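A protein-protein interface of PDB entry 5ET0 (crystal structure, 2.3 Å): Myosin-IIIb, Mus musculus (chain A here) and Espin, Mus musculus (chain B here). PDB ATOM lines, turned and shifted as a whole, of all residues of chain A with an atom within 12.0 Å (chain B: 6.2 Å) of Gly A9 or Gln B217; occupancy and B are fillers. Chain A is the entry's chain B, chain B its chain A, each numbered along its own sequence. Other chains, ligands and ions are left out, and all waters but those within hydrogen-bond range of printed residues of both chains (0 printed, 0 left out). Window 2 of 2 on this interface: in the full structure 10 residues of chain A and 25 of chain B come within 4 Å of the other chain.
Among the printed residues, pairs that only touch across the chains: Ile A11 with Gln B183 (3.7 Å), Gln A10 with Gln B217 (3.7 Å), Ile A11 with Met B218 (3.9 Å) and Ile A11 with Arg B252 (3.96 Å).
Of the printed residues of chain B, Ile A11 touches Gln B183, Met B218 and Arg B252. Of the printed residues of chain A, Tyr B179 touches Lys A12 (2.6 Å). Of chain A, only Ile A11 (3.7 Å) and Lys A12 (2.8 Å) come within 4 Å of Gln B183. Of the printed residues of chain A, Asp B207 touches Lys A12. No residue of chain A comes within 4 Å of Ala B214. Gln B217 touches just these residues of chain A: Gly A9 and Gln A10. Met B218 touches one residue of chain A. No residue of chain A comes within 4 Å of His B220. Ala B249 touches none of the printed residues of chain A. The nearest residue of chain B that does not touch Gly A9 is Phe B248 (4.2 Å). The nearest residue of chain A that does not touch Gln B217 is Ile A11 (4.2 Å). The nearest printed residue of chain A that does not touch Asp B207 is Gly A9 (4.4 Å).
Printed residues of chain B that touch a printed residue of chain A: Tyr B179, Gln B183, Asp B207, Met B209, Gln B217, Met B218 and Arg B252. Of the 5 printed residues of chain A, 4 touch a printed residue of chain B. Among the printed residues, 9 pairs touch across the chains.
SD of Met B209 lies within hydrogen-bond range of OH of Tyr B179 (3.7 Å). A ring nitrogen (NE2) of His B220 lies close to the backbone carbonyl oxygen (O) of Gln B183. N of Met B209 is in hydrogen-bond range of OD1 of Asp B207, at 3.1 Å. The backbone carbonyl oxygen of Gln B217 is in hydrogen-bond range of a ring nitrogen (NE2) of His B254 (2.8 Å). The backbone carbonyl oxygen of Gln A10 is in hydrogen-bond range of the side-chain amino group of Lys A12 (3.3 Å).
The side-chain hydroxyl of Tyr B179 lies within hydrogen-bond range of the side-chain amino group of Lys A12, 2.6 Å away. The side-chain amide oxygen (OE1) of Gln B183 lies within hydrogen-bond range of the backbone NH (N) of Lys A12. OD2 of Asp B207 is in salt-bridge range of NZ of Lys A12. The side-chain amino group (NZ) of Lys A12 is in hydrogen-bond range of the side-chain sulfur (SD) of Met B209 (3.2 Å). NE2 of Gln B217 is in hydrogen-bond range of O of Gly A9 (3.3 Å).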
ATOM      1  N   GLY A   9      -2.136 -20.383  -6.827  1.00  0.00           N
ATOM      2  CA  GLY A   9      -2.323 -21.185  -5.627  1.00  0.00           C
ATOM      3  C   GLY A   9      -2.719 -22.609  -5.969  1.00  0.00           C
ATOM      4  O   GLY A   9      -3.007 -22.919  -7.123  1.00  0.00           O
ATOM      5  N   GLN A  10      -2.722 -23.490  -4.975  1.00  0.00           N
ATOM      6  CA  GLN A  10      -3.100 -24.882  -5.176  1.00  0.00           C
ATOM      7  C   GLN A  10      -4.471 -25.140  -4.567  1.00  0.00           C
ATOM      8  O   GLN A  10      -4.983 -24.336  -3.787  1.00  0.00           O
ATOM      9  CB  GLN A  10      -2.069 -25.837  -4.578  1.00  0.00           C
ATOM     10  CG  GLN A  10      -0.739 -25.845  -5.308  1.00  0.00           C
ATOM     11  CD  GLN A  10       0.267 -26.765  -4.639  1.00  0.00           C
ATOM     12  OE1 GLN A  10       0.160 -27.044  -3.444  1.00  0.00           O
ATOM     13  NE2 GLN A  10       1.268 -27.217  -5.396  1.00  0.00           N
ATOM     14  N   ILE A  11      -5.097 -26.239  -4.976  1.00  0.00           N
ATOM     15  CA  ILE A  11      -6.383 -26.598  -4.399  1.00  0.00           C
ATOM     16  C   ILE A  11      -6.140 -27.298  -3.064  1.00  0.00           C
ATOM     17  O   ILE A  11      -5.148 -28.012  -2.884  1.00  0.00           O
ATOM     18  CB  ILE A  11      -7.182 -27.466  -5.381  1.00  0.00           C
ATOM     19  CG1 ILE A  11      -6.573 -28.859  -5.461  1.00  0.00           C
ATOM     20  CG2 ILE A  11      -7.130 -26.812  -6.761  1.00  0.00           C
ATOM     21  CD1 ILE A  11      -7.431 -29.887  -6.178  1.00  0.00           C
ATOM     22  N   LYS A  12      -7.024 -27.072  -2.102  1.00  0.00           N
ATOM     23  CA  LYS A  12      -6.859 -27.653  -0.781  1.00  0.00           C
ATOM     24  C   LYS A  12      -7.601 -28.977  -0.731  1.00  0.00           C
ATOM     25  O   LYS A  12      -8.818 -29.027  -0.950  1.00  0.00           O
ATOM     26  CB  LYS A  12      -7.354 -26.712   0.305  1.00  0.00           C
ATOM     27  CG  LYS A  12      -6.333 -25.648   0.712  1.00  0.00           C
ATOM     28  CD  LYS A  12      -6.027 -24.731  -0.413  1.00  0.00           C
ATOM     29  CE  LYS A  12      -5.503 -23.397   0.068  1.00  0.00           C
ATOM     30  NZ  LYS A  12      -5.536 -22.417  -1.103  1.00  0.00           N
ATOM     31  N   VAL A  13      -6.870 -30.039  -0.413  1.00  0.00           N
ATOM     32  CA  VAL A  13      -7.427 -31.381  -0.373  1.00  0.00           C
ATOM     33  C   VAL A  13      -7.342 -31.911   1.046  1.00  0.00           C
ATOM     34  O   VAL A  13      -6.514 -31.485   1.859  1.00  0.00           O
ATOM     35  CB  VAL A  13      -6.704 -32.339  -1.345  1.00  0.00           C
ATOM     36  CG1 VAL A  13      -6.610 -31.731  -2.755  1.00  0.00           C
ATOM     37  CG2 VAL A  13      -5.320 -32.726  -0.788  1.00  0.00           C
ATOM     38  N   TYR B 179     -14.356 -22.537   3.459  1.00  0.00           N
ATOM     39  CA  TYR B 179     -13.394 -22.594   2.370  1.00  0.00           C
ATOM     40  C   TYR B 179     -13.652 -23.816   1.500  1.00  0.00           C
ATOM     41  O   TYR B 179     -13.655 -23.732   0.263  1.00  0.00           O
ATOM     42  CB  TYR B 179     -11.958 -22.614   2.904  1.00  0.00           C
ATOM     43  CG  TYR B 179     -10.925 -22.495   1.799  1.00  0.00           C
ATOM     44  CD1 TYR B 179     -10.576 -23.596   1.000  1.00  0.00           C
ATOM     45  CD2 TYR B 179     -10.292 -21.289   1.546  1.00  0.00           C
ATOM     46  CE1 TYR B 179      -9.635 -23.479  -0.030  1.00  0.00           C
ATOM     47  CE2 TYR B 179      -9.355 -21.173   0.519  1.00  0.00           C
ATOM     48  CZ  TYR B 179      -9.022 -22.259  -0.238  1.00  0.00           C
ATOM     49  OH  TYR B 179      -8.108 -22.099  -1.251  1.00  0.00           O
ATOM     50  N   GLN B 183     -14.803 -23.810  -2.368  1.00  0.00           N
ATOM     51  CA  GLN B 183     -13.901 -24.413  -3.337  1.00  0.00           C
ATOM     52  C   GLN B 183     -14.616 -25.463  -4.158  1.00  0.00           C
ATOM     53  O   GLN B 183     -14.348 -25.627  -5.357  1.00  0.00           O
ATOM     54  CB  GLN B 183     -12.699 -25.050  -2.624  1.00  0.00           C
ATOM     55  CG  GLN B 183     -11.715 -25.805  -3.565  1.00  0.00           C
ATOM     56  CD  GLN B 183     -10.593 -26.537  -2.788  1.00  0.00           C
ATOM     57  OE1 GLN B 183      -9.555 -25.954  -2.474  1.00  0.00           O
ATOM     58  NE2 GLN B 183     -10.812 -27.813  -2.488  1.00  0.00           N
ATOM     59  N   ASP B 207      -2.021 -20.144   2.576  1.00  0.00           N
ATOM     60  CA  ASP B 207      -1.450 -19.364   1.494  1.00  0.00           C
ATOM     61  C   ASP B 207      -2.079 -17.989   1.367  1.00  0.00           C
ATOM     62  O   ASP B 207      -1.715 -17.240   0.469  1.00  0.00           O
ATOM     63  CB  ASP B 207      -1.568 -20.119   0.158  1.00  0.00           C
ATOM     64  CG  ASP B 207      -3.010 -20.435  -0.236  1.00  0.00           C
ATOM     65  OD1 ASP B 207      -3.947 -20.107   0.533  1.00  0.00           O
ATOM     66  OD2 ASP B 207      -3.198 -21.020  -1.332  1.00  0.00           O
ATOM     67  N   MET B 209      -5.375 -17.362   0.797  1.00  0.00           N
ATOM     68  CA  MET B 209      -6.636 -17.429   0.055  1.00  0.00           C
ATOM     69  C   MET B 209      -7.839 -17.468   0.990  1.00  0.00           C
ATOM     70  O   MET B 209      -7.824 -18.160   2.011  1.00  0.00           O
ATOM     71  CB  MET B 209      -6.648 -18.682  -0.827  1.00  0.00           C
ATOM     72  CG  MET B 209      -5.582 -18.610  -1.890  1.00  0.00           C
ATOM     73  SD  MET B 209      -5.684 -19.949  -3.056  1.00  0.00           S
ATOM     74  CE  MET B 209      -7.220 -19.582  -3.916  1.00  0.00           C
ATOM     75  N   LEU B 212     -13.689 -16.743  -0.976  1.00  0.00           N
ATOM     76  CA  LEU B 212     -13.996 -16.064  -2.226  1.00  0.00           C
ATOM     77  C   LEU B 212     -13.019 -16.453  -3.331  1.00  0.00           C
ATOM     78  O   LEU B 212     -13.424 -16.707  -4.469  1.00  0.00           O
ATOM     79  CB  LEU B 212     -13.955 -14.553  -2.017  1.00  0.00           C
ATOM     80  CG  LEU B 212     -14.316 -13.787  -3.310  1.00  0.00           C
ATOM     81  CD1 LEU B 212     -15.747 -14.053  -3.711  1.00  0.00           C
ATOM     82  CD2 LEU B 212     -14.075 -12.307  -3.095  1.00  0.00           C
ATOM     83  N   HIS B 213     -11.726 -16.481  -3.018  1.00  0.00           N
ATOM     84  CA  HIS B 213     -10.730 -16.890  -3.998  1.00  0.00           C
ATOM     85  C   HIS B 213     -10.910 -18.348  -4.393  1.00  0.00           C
ATOM     86  O   HIS B 213     -10.811 -18.697  -5.583  1.00  0.00           O
ATOM     87  CB  HIS B 213      -9.338 -16.663  -3.434  1.00  0.00           C
ATOM     88  CG  HIS B 213      -9.087 -15.248  -3.027  1.00  0.00           C
ATOM     89  ND1 HIS B 213      -8.474 -14.914  -1.836  1.00  0.00           N
ATOM     90  CD2 HIS B 213      -9.364 -14.082  -3.646  1.00  0.00           C
ATOM     91  CE1 HIS B 213      -8.373 -13.602  -1.749  1.00  0.00           C
ATOM     92  NE2 HIS B 213      -8.918 -13.071  -2.827  1.00  0.00           N
ATOM     93  N   ALA B 214     -11.168 -19.218  -3.412  1.00  0.00           N
ATOM     94  CA  ALA B 214     -11.394 -20.615  -3.757  1.00  0.00           C
ATOM     95  C   ALA B 214     -12.555 -20.755  -4.745  1.00  0.00           C
ATOM     96  O   ALA B 214     -12.474 -21.522  -5.711  1.00  0.00           O
ATOM     97  CB  ALA B 214     -11.654 -21.431  -2.486  1.00  0.00           C
ATOM     98  N   ALA B 215     -13.647 -20.015  -4.536  1.00  0.00           N
ATOM     99  CA  ALA B 215     -14.743 -20.103  -5.512  1.00  0.00           C
ATOM    100  C   ALA B 215     -14.318 -19.540  -6.869  1.00  0.00           C
ATOM    101  O   ALA B 215     -14.653 -20.103  -7.920  1.00  0.00           O
ATOM    102  CB  ALA B 215     -15.988 -19.390  -4.983  1.00  0.00           C
ATOM    103  N   ALA B 216     -13.550 -18.447  -6.869  1.00  0.00           N
ATOM    104  CA  ALA B 216     -13.099 -17.890  -8.143  1.00  0.00           C
ATOM    105  C   ALA B 216     -12.134 -18.842  -8.853  1.00  0.00           C
ATOM    106  O   ALA B 216     -12.248 -19.060 -10.069  1.00  0.00           O
ATOM    107  CB  ALA B 216     -12.459 -16.524  -7.908  1.00  0.00           C
ATOM    108  N   GLN B 217     -11.214 -19.449  -8.095  1.00  0.00           N
ATOM    109  CA  GLN B 217     -10.211 -20.351  -8.652  1.00  0.00           C
ATOM    110  C   GLN B 217     -10.858 -21.549  -9.336  1.00  0.00           C
ATOM    111  O   GLN B 217     -10.396 -21.986 -10.384  1.00  0.00           O
ATOM    112  CB  GLN B 217      -9.282 -20.822  -7.530  1.00  0.00           C
ATOM    113  CG  GLN B 217      -8.249 -21.863  -7.898  1.00  0.00           C
ATOM    114  CD  GLN B 217      -7.505 -22.378  -6.647  1.00  0.00           C
ATOM    115  OE1 GLN B 217      -8.126 -22.845  -5.694  1.00  0.00           O
ATOM    116  NE2 GLN B 217      -6.190 -22.288  -6.653  1.00  0.00           N
ATOM    117  N   MET B 218     -11.919 -22.096  -8.748  1.00  0.00           N
ATOM    118  CA  MET B 218     -12.559 -23.297  -9.274  1.00  0.00           C
ATOM    119  C   MET B 218     -13.740 -22.999 -10.181  1.00  0.00           C
ATOM    120  O   MET B 218     -14.411 -23.938 -10.604  1.00  0.00           O
ATOM    121  CB  MET B 218     -13.004 -24.224  -8.116  1.00  0.00           C
ATOM    122  CG  MET B 218     -11.808 -24.682  -7.226  1.00  0.00           C
ATOM    123  SD  MET B 218     -10.443 -25.374  -8.240  1.00  0.00           S
ATOM    124  CE  MET B 218     -11.300 -26.647  -9.162  1.00  0.00           C
ATOM    125  N   GLY B 219     -14.031 -21.727 -10.459  1.00  0.00           N
ATOM    126  CA  GLY B 219     -15.104 -21.338 -11.381  1.00  0.00           C
ATOM    127  C   GLY B 219     -16.528 -21.443 -10.869  1.00  0.00           C
ATOM    128  O   GLY B 219     -17.455 -21.570 -11.670  1.00  0.00           O
ATOM    129  N   HIS B 220     -16.749 -21.414  -9.546  1.00  0.00           N
ATOM    130  CA  HIS B 220     -18.094 -21.648  -9.015  1.00  0.00           C
ATOM    131  C   HIS B 220     -18.795 -20.306  -8.869  1.00  0.00           C
ATOM    132  O   HIS B 220     -18.948 -19.747  -7.766  1.00  0.00           O
ATOM    133  CB  HIS B 220     -18.029 -22.415  -7.703  1.00  0.00           C
ATOM    134  CG  HIS B 220     -17.415 -23.762  -7.857  1.00  0.00           C
ATOM    135  ND1 HIS B 220     -17.786 -24.629  -8.873  1.00  0.00           N
ATOM    136  CD2 HIS B 220     -16.436 -24.385  -7.150  1.00  0.00           C
ATOM    137  CE1 HIS B 220     -17.055 -25.728  -8.784  1.00  0.00           C
ATOM    138  NE2 HIS B 220     -16.242 -25.613  -7.737  1.00  0.00           N
ATOM    139  N   ASP B 239      -5.248 -12.028  -1.613  1.00  0.00           N
ATOM    140  CA  ASP B 239      -4.436 -13.038  -0.939  1.00  0.00           C
ATOM    141  C   ASP B 239      -3.085 -12.428  -0.568  1.00  0.00           C
ATOM    142  O   ASP B 239      -2.861 -11.230  -0.746  1.00  0.00           O
ATOM    143  CB  ASP B 239      -4.321 -14.304  -1.797  1.00  0.00           C
ATOM    144  CG  ASP B 239      -3.247 -14.215  -2.896  1.00  0.00           C
ATOM    145  OD1 ASP B 239      -2.784 -13.108  -3.254  1.00  0.00           O
ATOM    146  OD2 ASP B 239      -2.891 -15.287  -3.424  1.00  0.00           O
ATOM    147  N   ALA B 245     -10.056 -12.127  -6.653  1.00  0.00           N
ATOM    148  CA  ALA B 245     -10.911 -13.111  -7.307  1.00  0.00           C
ATOM    149  C   ALA B 245     -10.754 -13.052  -8.820  1.00  0.00           C
ATOM    150  O   ALA B 245     -10.830 -14.077  -9.491  1.00  0.00           O
ATOM    151  CB  ALA B 245     -12.378 -12.892  -6.935  1.00  0.00           C
ATOM    152  N   PHE B 248      -7.622 -15.022 -10.019  1.00  0.00           N
ATOM    153  CA  PHE B 248      -7.780 -16.481  -9.942  1.00  0.00           C
ATOM    154  C   PHE B 248      -8.707 -16.983 -11.047  1.00  0.00           C
ATOM    155  O   PHE B 248      -8.407 -17.980 -11.710  1.00  0.00           O
ATOM    156  CB  PHE B 248      -8.303 -16.923  -8.552  1.00  0.00           C
ATOM    157  CG  PHE B 248      -7.260 -16.879  -7.430  1.00  0.00           C
ATOM    158  CD1 PHE B 248      -6.354 -17.911  -7.242  1.00  0.00           C
ATOM    159  CD2 PHE B 248      -7.201 -15.817  -6.571  1.00  0.00           C
ATOM    160  CE1 PHE B 248      -5.408 -17.877  -6.237  1.00  0.00           C
ATOM    161  CE2 PHE B 248      -6.254 -15.773  -5.537  1.00  0.00           C
ATOM    162  CZ  PHE B 248      -5.356 -16.798  -5.367  1.00  0.00           C
ATOM    163  N   ALA B 249      -9.817 -16.284 -11.291  1.00  0.00           N
ATOM    164  CA  ALA B 249     -10.682 -16.644 -12.414  1.00  0.00           C
ATOM    165  C   ALA B 249      -9.917 -16.596 -13.738  1.00  0.00           C
ATOM    166  O   ALA B 249      -9.915 -17.570 -14.503  1.00  0.00           O
ATOM    167  CB  ALA B 249     -11.900 -15.718 -12.469  1.00  0.00           C
ATOM    168  N   ARG B 252      -7.286 -19.378 -14.354  1.00  0.00           N
ATOM    169  CA  ARG B 252      -7.768 -20.738 -14.516  1.00  0.00           C
ATOM    170  C   ARG B 252      -8.860 -20.816 -15.574  1.00  0.00           C
ATOM    171  O   ARG B 252      -9.559 -21.833 -15.671  1.00  0.00           O
ATOM    172  CB  ARG B 252      -8.247 -21.288 -13.174  1.00  0.00           C
ATOM    173  CG  ARG B 252      -7.112 -22.075 -12.463  1.00  0.00           C
ATOM    174  CD  ARG B 252      -7.583 -22.725 -11.224  1.00  0.00           C
ATOM    175  NE  ARG B 252      -6.734 -23.843 -10.802  1.00  0.00           N
ATOM    176  CZ  ARG B 252      -7.083 -25.109 -10.971  1.00  0.00           C
ATOM    177  NH1 ARG B 252      -8.233 -25.398 -11.572  1.00  0.00           N
ATOM    178  NH2 ARG B 252      -6.291 -26.078 -10.564  1.00  0.00           N
ATOM    179  N   HIS B 254     -11.826 -19.129 -16.102  1.00  0.00           N
ATOM    180  CA  HIS B 254     -13.253 -19.133 -15.723  1.00  0.00           C
ATOM    181  C   HIS B 254     -13.965 -17.887 -16.243  1.00  0.00           C
ATOM    182  O   HIS B 254     -14.261 -16.924 -15.515  1.00  0.00           O
ATOM    183  CB  HIS B 254     -13.369 -19.283 -14.212  1.00  0.00           C
ATOM    184  CG  HIS B 254     -12.833 -20.600 -13.732  1.00  0.00           C
ATOM    185  ND1 HIS B 254     -13.072 -21.773 -14.412  1.00  0.00           N
ATOM    186  CD2 HIS B 254     -12.025 -20.927 -12.692  1.00  0.00           C
ATOM    187  CE1 HIS B 254     -12.477 -22.775 -13.790  1.00  0.00           C
ATOM    188  NE2 HIS B 254     -11.841 -22.291 -12.740  1.00  0.00           N
